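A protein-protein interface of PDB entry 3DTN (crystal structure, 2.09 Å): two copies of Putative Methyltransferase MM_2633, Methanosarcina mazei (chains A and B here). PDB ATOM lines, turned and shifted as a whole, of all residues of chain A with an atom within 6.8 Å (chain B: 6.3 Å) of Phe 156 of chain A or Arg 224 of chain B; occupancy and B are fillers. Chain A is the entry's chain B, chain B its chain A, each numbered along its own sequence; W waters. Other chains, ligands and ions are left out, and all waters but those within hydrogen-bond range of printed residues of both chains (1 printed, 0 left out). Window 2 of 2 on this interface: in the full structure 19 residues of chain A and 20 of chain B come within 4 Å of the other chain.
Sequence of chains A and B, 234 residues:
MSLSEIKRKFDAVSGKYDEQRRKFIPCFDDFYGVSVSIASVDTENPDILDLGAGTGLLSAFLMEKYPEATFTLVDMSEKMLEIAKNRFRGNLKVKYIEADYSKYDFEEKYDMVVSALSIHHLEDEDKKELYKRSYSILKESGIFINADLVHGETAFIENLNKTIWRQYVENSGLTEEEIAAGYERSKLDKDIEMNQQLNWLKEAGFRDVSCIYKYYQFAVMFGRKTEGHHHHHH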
ATOM      1  N   GLY A 152     -12.737  10.082 -26.931  1.00  0.00           N
ATOM      2  CA  GLY A 152     -12.752  11.284 -26.092  1.00  0.00           C
ATOM      3  C   GLY A 152     -12.763  10.977 -24.604  1.00  0.00           C
ATOM      4  O   GLY A 152     -13.289   9.951 -24.180  1.00  0.00           O
ATOM      5  N   GLU A 153     -12.133  11.854 -23.823  1.00  0.00           N
ATOM      6  CA  GLU A 153     -11.952  11.665 -22.403  1.00  0.00           C
ATOM      7  C   GLU A 153     -13.285  11.826 -21.686  1.00  0.00           C
ATOM      8  O   GLU A 153     -13.487  11.265 -20.628  1.00  0.00           O
ATOM      9  CB  GLU A 153     -10.920  12.716 -21.878  1.00  0.00           C
ATOM     10  CG  GLU A 153      -9.450  12.311 -22.108  1.00  0.00           C
ATOM     11  CD  GLU A 153      -8.978  12.541 -23.529  1.00  0.00           C
ATOM     12  OE1 GLU A 153      -9.699  13.228 -24.290  1.00  0.00           O
ATOM     13  OE2 GLU A 153      -7.874  12.060 -23.899  1.00  0.00           O
ATOM     14  N   THR A 154     -14.197  12.618 -22.246  1.00  0.00           N
ATOM     15  CA  THR A 154     -15.591  12.708 -21.734  1.00  0.00           C
ATOM     16  C   THR A 154     -16.503  12.666 -22.973  1.00  0.00           C
ATOM     17  O   THR A 154     -15.994  12.718 -24.093  1.00  0.00           O
ATOM     18  CB  THR A 154     -15.839  14.003 -20.986  1.00  0.00           C
ATOM     19  OG1 THR A 154     -15.679  15.125 -21.888  1.00  0.00           O
ATOM     20  CG2 THR A 154     -14.863  14.113 -19.756  1.00  0.00           C
ATOM     21  N   ALA A 155     -17.824  12.557 -22.773  1.00  0.00           N
ATOM     22  CA  ALA A 155     -18.776  12.590 -23.867  1.00  0.00           C
ATOM     23  C   ALA A 155     -18.701  13.871 -24.669  1.00  0.00           C
ATOM     24  O   ALA A 155     -18.846  13.859 -25.857  1.00  0.00           O
ATOM     25  CB  ALA A 155     -20.236  12.374 -23.335  1.00  0.00           C
ATOM     26  N   PHE A 156     -18.492  15.001 -24.021  1.00  0.00           N
ATOM     27  CA  PHE A 156     -18.309  16.257 -24.751  1.00  0.00           C
ATOM     28  C   PHE A 156     -17.086  16.207 -25.705  1.00  0.00           C
ATOM     29  O   PHE A 156     -17.173  16.645 -26.855  1.00  0.00           O
ATOM     30  CB  PHE A 156     -18.183  17.408 -23.740  1.00  0.00           C
ATOM     31  CG  PHE A 156     -17.884  18.747 -24.366  1.00  0.00           C
ATOM     32  CD1 PHE A 156     -18.908  19.600 -24.737  1.00  0.00           C
ATOM     33  CD2 PHE A 156     -16.554  19.155 -24.573  1.00  0.00           C
ATOM     34  CE1 PHE A 156     -18.629  20.837 -25.312  1.00  0.00           C
ATOM     35  CE2 PHE A 156     -16.252  20.396 -25.153  1.00  0.00           C
ATOM     36  CZ  PHE A 156     -17.285  21.247 -25.528  1.00  0.00           C
ATOM     37  N   ILE A 157     -15.954  15.681 -25.231  1.00  0.00           N
ATOM     38  CA  ILE A 157     -14.744  15.601 -26.052  1.00  0.00           C
ATOM     39  C   ILE A 157     -14.943  14.576 -27.181  1.00  0.00           C
ATOM     40  O   ILE A 157     -14.513  14.791 -28.319  1.00  0.00           O
ATOM     41  CB  ILE A 157     -13.485  15.274 -25.195  1.00  0.00           C
ATOM     42  CG1 ILE A 157     -13.230  16.438 -24.212  1.00  0.00           C
ATOM     43  CG2 ILE A 157     -12.221  15.070 -26.122  1.00  0.00           C
ATOM     44  CD1 ILE A 157     -12.844  17.751 -24.925  1.00  0.00           C
ATOM     45  N   GLU A 158     -15.588  13.453 -26.877  1.00  0.00           N
ATOM     46  CA  GLU A 158     -15.926  12.494 -27.950  1.00  0.00           C
ATOM     47  C   GLU A 158     -16.727  13.187 -29.070  1.00  0.00           C
ATOM     48  O   GLU A 158     -16.374  13.082 -30.236  1.00  0.00           O
ATOM     49  CB  GLU A 158     -16.676  11.268 -27.375  1.00  0.00           C
ATOM     50  CG  GLU A 158     -17.216  10.337 -28.446  1.00  0.00           C
ATOM     51  CD  GLU A 158     -16.066   9.627 -29.191  1.00  0.00           C
ATOM     52  OE1 GLU A 158     -14.890   9.758 -28.765  1.00  0.00           O
ATOM     53  OE2 GLU A 158     -16.341   8.948 -30.192  1.00  0.00           O
ATOM     54  N   ASN A 159     -17.817  13.883 -28.708  1.00  0.00           N
ATOM     55  CA  ASN A 159     -18.603  14.668 -29.660  1.00  0.00           C
ATOM     56  C   ASN A 159     -17.785  15.711 -30.410  1.00  0.00           C
ATOM     57  O   ASN A 159     -17.949  15.848 -31.608  1.00  0.00           O
ATOM     58  CB  ASN A 159     -19.762  15.399 -28.970  1.00  0.00           C
ATOM     59  CG  ASN A 159     -20.783  14.443 -28.460  1.00  0.00           C
ATOM     60  OD1 ASN A 159     -21.588  14.751 -27.549  1.00  0.00           O
ATOM     61  ND2 ASN A 159     -20.760  13.237 -29.038  1.00  0.00           N
ATOM     62  N   LEU A 160     -16.935  16.449 -29.692  1.00  0.00           N
ATOM     63  CA  LEU A 160     -16.014  17.392 -30.324  1.00  0.00           C
ATOM     64  C   LEU A 160     -15.168  16.685 -31.400  1.00  0.00           C
ATOM     65  O   LEU A 160     -15.127  17.108 -32.564  1.00  0.00           O
ATOM     66  CB  LEU A 160     -15.114  18.052 -29.291  1.00  0.00           C
ATOM     67  CG  LEU A 160     -13.989  18.929 -29.892  1.00  0.00           C
ATOM     68  CD1 LEU A 160     -14.578  20.132 -30.640  1.00  0.00           C
ATOM     69  CD2 LEU A 160     -13.096  19.431 -28.758  1.00  0.00           C
ATOM     70  N   ASN A 161     -14.549  15.570 -31.023  1.00  0.00           N
ATOM     71  CA  ASN A 161     -13.681  14.850 -31.946  1.00  0.00           C
ATOM     72  C   ASN A 161     -14.467  14.361 -33.162  1.00  0.00           C
ATOM     73  O   ASN A 161     -14.026  14.513 -34.292  1.00  0.00           O
ATOM     74  CB  ASN A 161     -13.016  13.614 -31.278  1.00  0.00           C
ATOM     75  CG  ASN A 161     -11.944  13.972 -30.223  1.00  0.00           C
ATOM     76  OD1 ASN A 161     -11.551  15.139 -30.053  1.00  0.00           O
ATOM     77  ND2 ASN A 161     -11.476  12.940 -29.498  1.00  0.00           N
ATOM     78  N   SER B  40     -15.181  27.517 -29.089  1.00  0.00           N
ATOM     79  CA  SER B  40     -16.543  27.667 -29.548  1.00  0.00           C
ATOM     80  C   SER B  40     -17.406  27.941 -28.358  1.00  0.00           C
ATOM     81  O   SER B  40     -17.391  27.183 -27.410  1.00  0.00           O
ATOM     82  CB  SER B  40     -17.008  26.380 -30.200  1.00  0.00           C
ATOM     83  OG  SER B  40     -16.215  26.146 -31.326  1.00  0.00           O
ATOM     84  N   TYR B 135      -9.874  29.499 -13.925  1.00  0.00           N
ATOM     85  CA  TYR B 135     -11.172  28.930 -13.593  1.00  0.00           C
ATOM     86  C   TYR B 135     -12.123  29.957 -12.963  1.00  0.00           C
ATOM     87  O   TYR B 135     -13.304  30.046 -13.339  1.00  0.00           O
ATOM     88  CB  TYR B 135     -11.026  27.692 -12.682  1.00  0.00           C
ATOM     89  CG  TYR B 135     -12.334  26.936 -12.497  1.00  0.00           C
ATOM     90  CD1 TYR B 135     -12.764  26.024 -13.458  1.00  0.00           C
ATOM     91  CD2 TYR B 135     -13.173  27.187 -11.398  1.00  0.00           C
ATOM     92  CE1 TYR B 135     -13.941  25.370 -13.346  1.00  0.00           C
ATOM     93  CE2 TYR B 135     -14.360  26.511 -11.269  1.00  0.00           C
ATOM     94  CZ  TYR B 135     -14.733  25.600 -12.243  1.00  0.00           C
ATOM     95  OH  TYR B 135     -15.916  24.914 -12.148  1.00  0.00           O
ATOM     96  N   LEU B 138     -13.710  32.735 -15.467  1.00  0.00           N
ATOM     97  CA  LEU B 138     -14.463  32.288 -16.622  1.00  0.00           C
ATOM     98  C   LEU B 138     -15.982  32.365 -16.352  1.00  0.00           C
ATOM     99  O   LEU B 138     -16.394  32.172 -15.233  1.00  0.00           O
ATOM    100  CB  LEU B 138     -14.054  30.847 -16.958  1.00  0.00           C
ATOM    101  CG  LEU B 138     -12.811  30.703 -17.858  1.00  0.00           C
ATOM    102  CD1 LEU B 138     -12.494  29.209 -17.920  1.00  0.00           C
ATOM    103  CD2 LEU B 138     -13.118  31.259 -19.230  1.00  0.00           C
ATOM    104  N   SER B 141     -19.886  27.620 -18.726  1.00  0.00           N
ATOM    105  CA  SER B 141     -19.547  27.063 -20.054  1.00  0.00           C
ATOM    106  C   SER B 141     -18.371  27.748 -20.751  1.00  0.00           C
ATOM    107  O   SER B 141     -18.189  27.576 -21.983  1.00  0.00           O
ATOM    108  CB  SER B 141     -20.751  27.062 -21.014  1.00  0.00           C
ATOM    109  OG  SER B 141     -21.780  26.224 -20.509  1.00  0.00           O
ATOM    110  N   GLY B 142     -17.623  28.572 -20.006  1.00  0.00           N
ATOM    111  CA  GLY B 142     -16.463  29.207 -20.603  1.00  0.00           C
ATOM    112  C   GLY B 142     -15.349  28.196 -20.829  1.00  0.00           C
ATOM    113  O   GLY B 142     -15.342  27.100 -20.237  1.00  0.00           O
ATOM    114  N   ILE B 143     -14.390  28.532 -21.671  1.00  0.00           N
ATOM    115  CA  ILE B 143     -13.346  27.551 -21.933  1.00  0.00           C
ATOM    116  C   ILE B 143     -11.940  28.096 -21.714  1.00  0.00           C
ATOM    117  O   ILE B 143     -11.699  29.300 -21.830  1.00  0.00           O
ATOM    118  CB  ILE B 143     -13.466  26.938 -23.327  1.00  0.00           C
ATOM    119  CG1 ILE B 143     -13.319  28.009 -24.399  1.00  0.00           C
ATOM    120  CG2 ILE B 143     -14.832  26.169 -23.492  1.00  0.00           C
ATOM    121  CD1 ILE B 143     -13.819  27.508 -25.735  1.00  0.00           C
ATOM    122  N   PHE B 144     -11.037  27.191 -21.360  1.00  0.00           N
ATOM    123  CA  PHE B 144      -9.635  27.487 -21.236  1.00  0.00           C
ATOM    124  C   PHE B 144      -8.863  26.745 -22.343  1.00  0.00           C
ATOM    125  O   PHE B 144      -9.032  25.525 -22.515  1.00  0.00           O
ATOM    126  CB  PHE B 144      -9.143  27.028 -19.854  1.00  0.00           C
ATOM    127  CG  PHE B 144      -7.661  27.267 -19.643  1.00  0.00           C
ATOM    128  CD1 PHE B 144      -7.202  28.502 -19.205  1.00  0.00           C
ATOM    129  CD2 PHE B 144      -6.731  26.276 -19.946  1.00  0.00           C
ATOM    130  CE1 PHE B 144      -5.853  28.743 -19.031  1.00  0.00           C
ATOM    131  CE2 PHE B 144      -5.356  26.515 -19.746  1.00  0.00           C
ATOM    132  CZ  PHE B 144      -4.934  27.749 -19.294  1.00  0.00           C
ATOM    133  N   GLY B 205     -10.680  22.587 -11.188  1.00  0.00           N
ATOM    134  CA  GLY B 205     -12.121  22.462 -11.321  1.00  0.00           C
ATOM    135  C   GLY B 205     -12.590  22.283 -12.768  1.00  0.00           C
ATOM    136  O   GLY B 205     -13.745  22.004 -13.029  1.00  0.00           O
ATOM    137  N   PHE B 206     -11.693  22.437 -13.730  1.00  0.00           N
ATOM    138  CA  PHE B 206     -12.086  22.222 -15.114  1.00  0.00           C
ATOM    139  C   PHE B 206     -12.592  20.814 -15.399  1.00  0.00           C
ATOM    140  O   PHE B 206     -12.109  19.836 -14.826  1.00  0.00           O
ATOM    141  CB  PHE B 206     -10.913  22.546 -16.046  1.00  0.00           C
ATOM    142  CG  PHE B 206     -10.631  23.991 -16.150  1.00  0.00           C
ATOM    143  CD1 PHE B 206     -11.364  24.776 -17.013  1.00  0.00           C
ATOM    144  CD2 PHE B 206      -9.615  24.578 -15.395  1.00  0.00           C
ATOM    145  CE1 PHE B 206     -11.115  26.145 -17.115  1.00  0.00           C
ATOM    146  CE2 PHE B 206      -9.339  25.960 -15.482  1.00  0.00           C
ATOM    147  CZ  PHE B 206     -10.086  26.752 -16.331  1.00  0.00           C
ATOM    148  N   ARG B 207     -13.563  20.724 -16.309  1.00  0.00           N
ATOM    149  CA  ARG B 207     -14.061  19.445 -16.841  1.00  0.00           C
ATOM    150  C   ARG B 207     -13.718  19.344 -18.316  1.00  0.00           C
ATOM    151  O   ARG B 207     -13.328  20.344 -18.958  1.00  0.00           O
ATOM    152  CB  ARG B 207     -15.604  19.382 -16.738  1.00  0.00           C
ATOM    153  CG  ARG B 207     -16.150  19.754 -15.399  1.00  0.00           C
ATOM    154  CD  ARG B 207     -15.623  18.844 -14.295  1.00  0.00           C
ATOM    155  NE  ARG B 207     -16.196  17.504 -14.401  1.00  0.00           N
ATOM    156  CZ  ARG B 207     -15.647  16.396 -13.894  1.00  0.00           C
ATOM    157  NH1 ARG B 207     -14.497  16.442 -13.230  1.00  0.00           N
ATOM    158  NH2 ARG B 207     -16.263  15.234 -14.048  1.00  0.00           N
ATOM    159  N   ASP B 208     -13.867  18.132 -18.848  1.00  0.00           N
ATOM    160  CA  ASP B 208     -13.635  17.850 -20.257  1.00  0.00           C
ATOM    161  C   ASP B 208     -12.209  18.215 -20.587  1.00  0.00           C
ATOM    162  O   ASP B 208     -11.915  18.662 -21.695  1.00  0.00           O
ATOM    163  CB  ASP B 208     -14.562  18.679 -21.117  1.00  0.00           C
ATOM    164  CG  ASP B 208     -16.022  18.411 -20.805  1.00  0.00           C
ATOM    165  OD1 ASP B 208     -16.402  17.214 -20.820  1.00  0.00           O
ATOM    166  OD2 ASP B 208     -16.772  19.396 -20.589  1.00  0.00           O
ATOM    167  N   VAL B 209     -11.334  18.058 -19.600  1.00  0.00           N
ATOM    168  CA  VAL B 209      -9.917  18.336 -19.778  1.00  0.00           C
ATOM    169  C   VAL B 209      -9.278  17.312 -20.736  1.00  0.00           C
ATOM    170  O   VAL B 209      -9.378  16.093 -20.541  1.00  0.00           O
ATOM    171  CB  VAL B 209      -9.205  18.344 -18.451  1.00  0.00           C
ATOM    172  CG1 VAL B 209      -7.632  18.420 -18.643  1.00  0.00           C
ATOM    173  CG2 VAL B 209      -9.779  19.499 -17.571  1.00  0.00           C
ATOM    174  N   PHE B 222      -7.049  21.770 -23.306  1.00  0.00           N
ATOM    175  CA  PHE B 222      -8.400  22.316 -23.321  1.00  0.00           C
ATOM    176  C   PHE B 222      -9.050  21.975 -21.985  1.00  0.00           C
ATOM    177  O   PHE B 222      -8.807  20.920 -21.421  1.00  0.00           O
ATOM    178  CB  PHE B 222      -9.237  21.640 -24.455  1.00  0.00           C
ATOM    179  CG  PHE B 222     -10.692  22.095 -24.503  1.00  0.00           C
ATOM    180  CD1 PHE B 222     -11.049  23.294 -25.143  1.00  0.00           C
ATOM    181  CD2 PHE B 222     -11.696  21.337 -23.884  1.00  0.00           C
ATOM    182  CE1 PHE B 222     -12.383  23.696 -25.194  1.00  0.00           C
ATOM    183  CE2 PHE B 222     -13.018  21.733 -23.896  1.00  0.00           C
ATOM    184  CZ  PHE B 222     -13.376  22.944 -24.563  1.00  0.00           C
ATOM    185  N   GLY B 223      -9.873  22.859 -21.466  1.00  0.00           N
ATOM    186  CA  GLY B 223     -10.665  22.514 -20.320  1.00  0.00           C
ATOM    187  C   GLY B 223     -11.893  23.406 -20.397  1.00  0.00           C
ATOM    188  O   GLY B 223     -11.889  24.439 -21.079  1.00  0.00           O
ATOM    189  N   ARG B 224     -12.937  23.032 -19.677  1.00  0.00           N
ATOM    190  CA  ARG B 224     -14.170  23.812 -19.722  1.00  0.00           C
ATOM    191  C   ARG B 224     -14.770  23.948 -18.325  1.00  0.00           C
ATOM    192  O   ARG B 224     -14.675  23.028 -17.518  1.00  0.00           O
ATOM    193  CB  ARG B 224     -15.084  23.038 -20.624  1.00  0.00           C
ATOM    194  CG  ARG B 224     -16.480  23.402 -20.678  1.00  0.00           C
ATOM    195  CD  ARG B 224     -16.968  22.389 -21.736  1.00  0.00           C
ATOM    196  NE  ARG B 224     -18.284  22.675 -22.237  1.00  0.00           N
ATOM    197  CZ  ARG B 224     -19.350  21.924 -22.008  1.00  0.00           C
ATOM    198  NH1 ARG B 224     -19.268  20.810 -21.281  1.00  0.00           N
ATOM    199  NH2 ARG B 224     -20.507  22.301 -22.528  1.00  0.00           N
ATOM    200  N   LYS B 225     -15.364  25.103 -18.045  1.00  0.00           N
ATOM    201  CA  LYS B 225     -16.064  25.351 -16.798  1.00  0.00           C
ATOM    202  C   LYS B 225     -17.564  25.098 -16.955  1.00  0.00           C
ATOM    203  O   LYS B 225     -18.251  25.805 -17.695  1.00  0.00           O
ATOM    204  CB  LYS B 225     -15.844  26.797 -16.352  1.00  0.00           C
ATOM    205  CG  LYS B 225     -16.664  27.213 -15.137  1.00  0.00           C
ATOM    206  CD  LYS B 225     -16.038  28.430 -14.563  1.00  0.00           C
ATOM    207  CE  LYS B 225     -16.691  28.878 -13.297  1.00  0.00           C
ATOM    208  NZ  LYS B 225     -16.091  30.189 -12.903  1.00  0.00           N
ATOM    209  N   THR B 226     -18.073  24.080 -16.259  1.00  0.00           N
ATOM    210  CA  THR B 226     -19.515  23.790 -16.289  1.00  0.00           C
ATOM    211  C   THR B 226     -20.016  23.314 -14.934  1.00  0.00           C
ATOM    212  O   THR B 226     -20.148  24.146 -14.018  1.00  0.00           O
ATOM    213  CB  THR B 226     -19.894  22.769 -17.392  1.00  0.00           C
ATOM    214  OG1 THR B 226     -19.167  21.558 -17.183  1.00  0.00           O
ATOM    215  CG2 THR B 226     -19.507  23.306 -18.753  1.00  0.00           C
HETATM  216  O   HOH W   1     -19.080  15.578 -21.156  1.00  0.00           O
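The side-chain carboxylate (OD1) of Asp 208 of chain B is in hydrogen-bond range of the side-chain hydroxyl (OG1) of Thr 154 of chain A (2.5 Å).
The backbone NH of Arg 224 of chain B sits at hydrogen-bond distance from the backbone carbonyl oxygen of Arg 207 of chain B (2.8 Å). The side-chain hydroxyl (OG1) of Thr 154 of chain A lies within hydrogen-bond range of the backbone NH (N) of Ile 157 of chain A, at 3.4 Å. The side-chain amide oxygen (OD1) of Asn 161 of chain A sits close to the backbone carbonyl oxygen (O) of Ile 157 of chain A, at 3.4 Å. OD2 of Asp 208 of chain B is in salt-bridge range of NH1 of Arg 224 of chain B, 3.0 Å away.
Among the printed residues, merely in contact across the chains: Phe 156 of chain A with Asp 208 of chain B, Ile 157 of chain A with Asp 208 of chain B, Phe 156 of chain A with Arg 224 of chain B, Phe 156 of chain A with Phe 222 of chain B, Ile 157 of chain A with Phe 222 of chain B and Glu 153 of chain A with Val 209 of chain B.
Phe 156 of chain A touches just these residues of chain B: Asp 208, Phe 222 and Arg 224. Of the printed residues of chain A, Arg 224 of chain B touches Phe 156 (3.6 Å). Printed residues of chain B within 4 Å of Ile 157 of chain A: Asp 208 (3.5 Å) and Phe 222 (3.9 Å). Of the printed residues of chain B, Glu 153 of chain A touches Val 209. Of the printed residues of chain B, Thr 154 of chain A touches Asp 208. Printed residues of chain A within 4 Å of Phe 222 of chain B: Phe 156 and Ile 157. Printed residues of chain A within 4 Å of Val 209 of chain B: Glu 153 (3.9 Å). The nearest residue of chain B that does not touch Phe 156 of chain A is Ile 143 of chain B (5.9 Å). The nearest printed residue of chain A that does not touch Arg 224 of chain B is Thr 154 of chain A (6.8 Å). The nearest printed residue of chain B that does not touch Ile 157 of chain A is Val 209 of chain B (5.2 Å).
Along chain B the printed residues that touch a printed residue of chain A span positions 208 to 224. Hydrophobic or aromatic side chains of chain A within 4 Å of the printed part of chain B: Phe 156 and Ile 157. Among the printed residues, 7 pairs touch across the chains. Among the printed residues, no Asp or Glu carboxylate lies within 4 Å of a Lys or Arg side-chain nitrogen of the other chain.
No position is printed for both chains. Of the 7 pairs that touch across the chains among the printed residues, none has its exchanged pair printed and touching as well.
Water W1 bridges the backbone NH (N) of Phe 156 of chain A (3.0 Å) and the side-chain carboxylate (OD1) of Asp 208 of chain B (3.2 Å).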
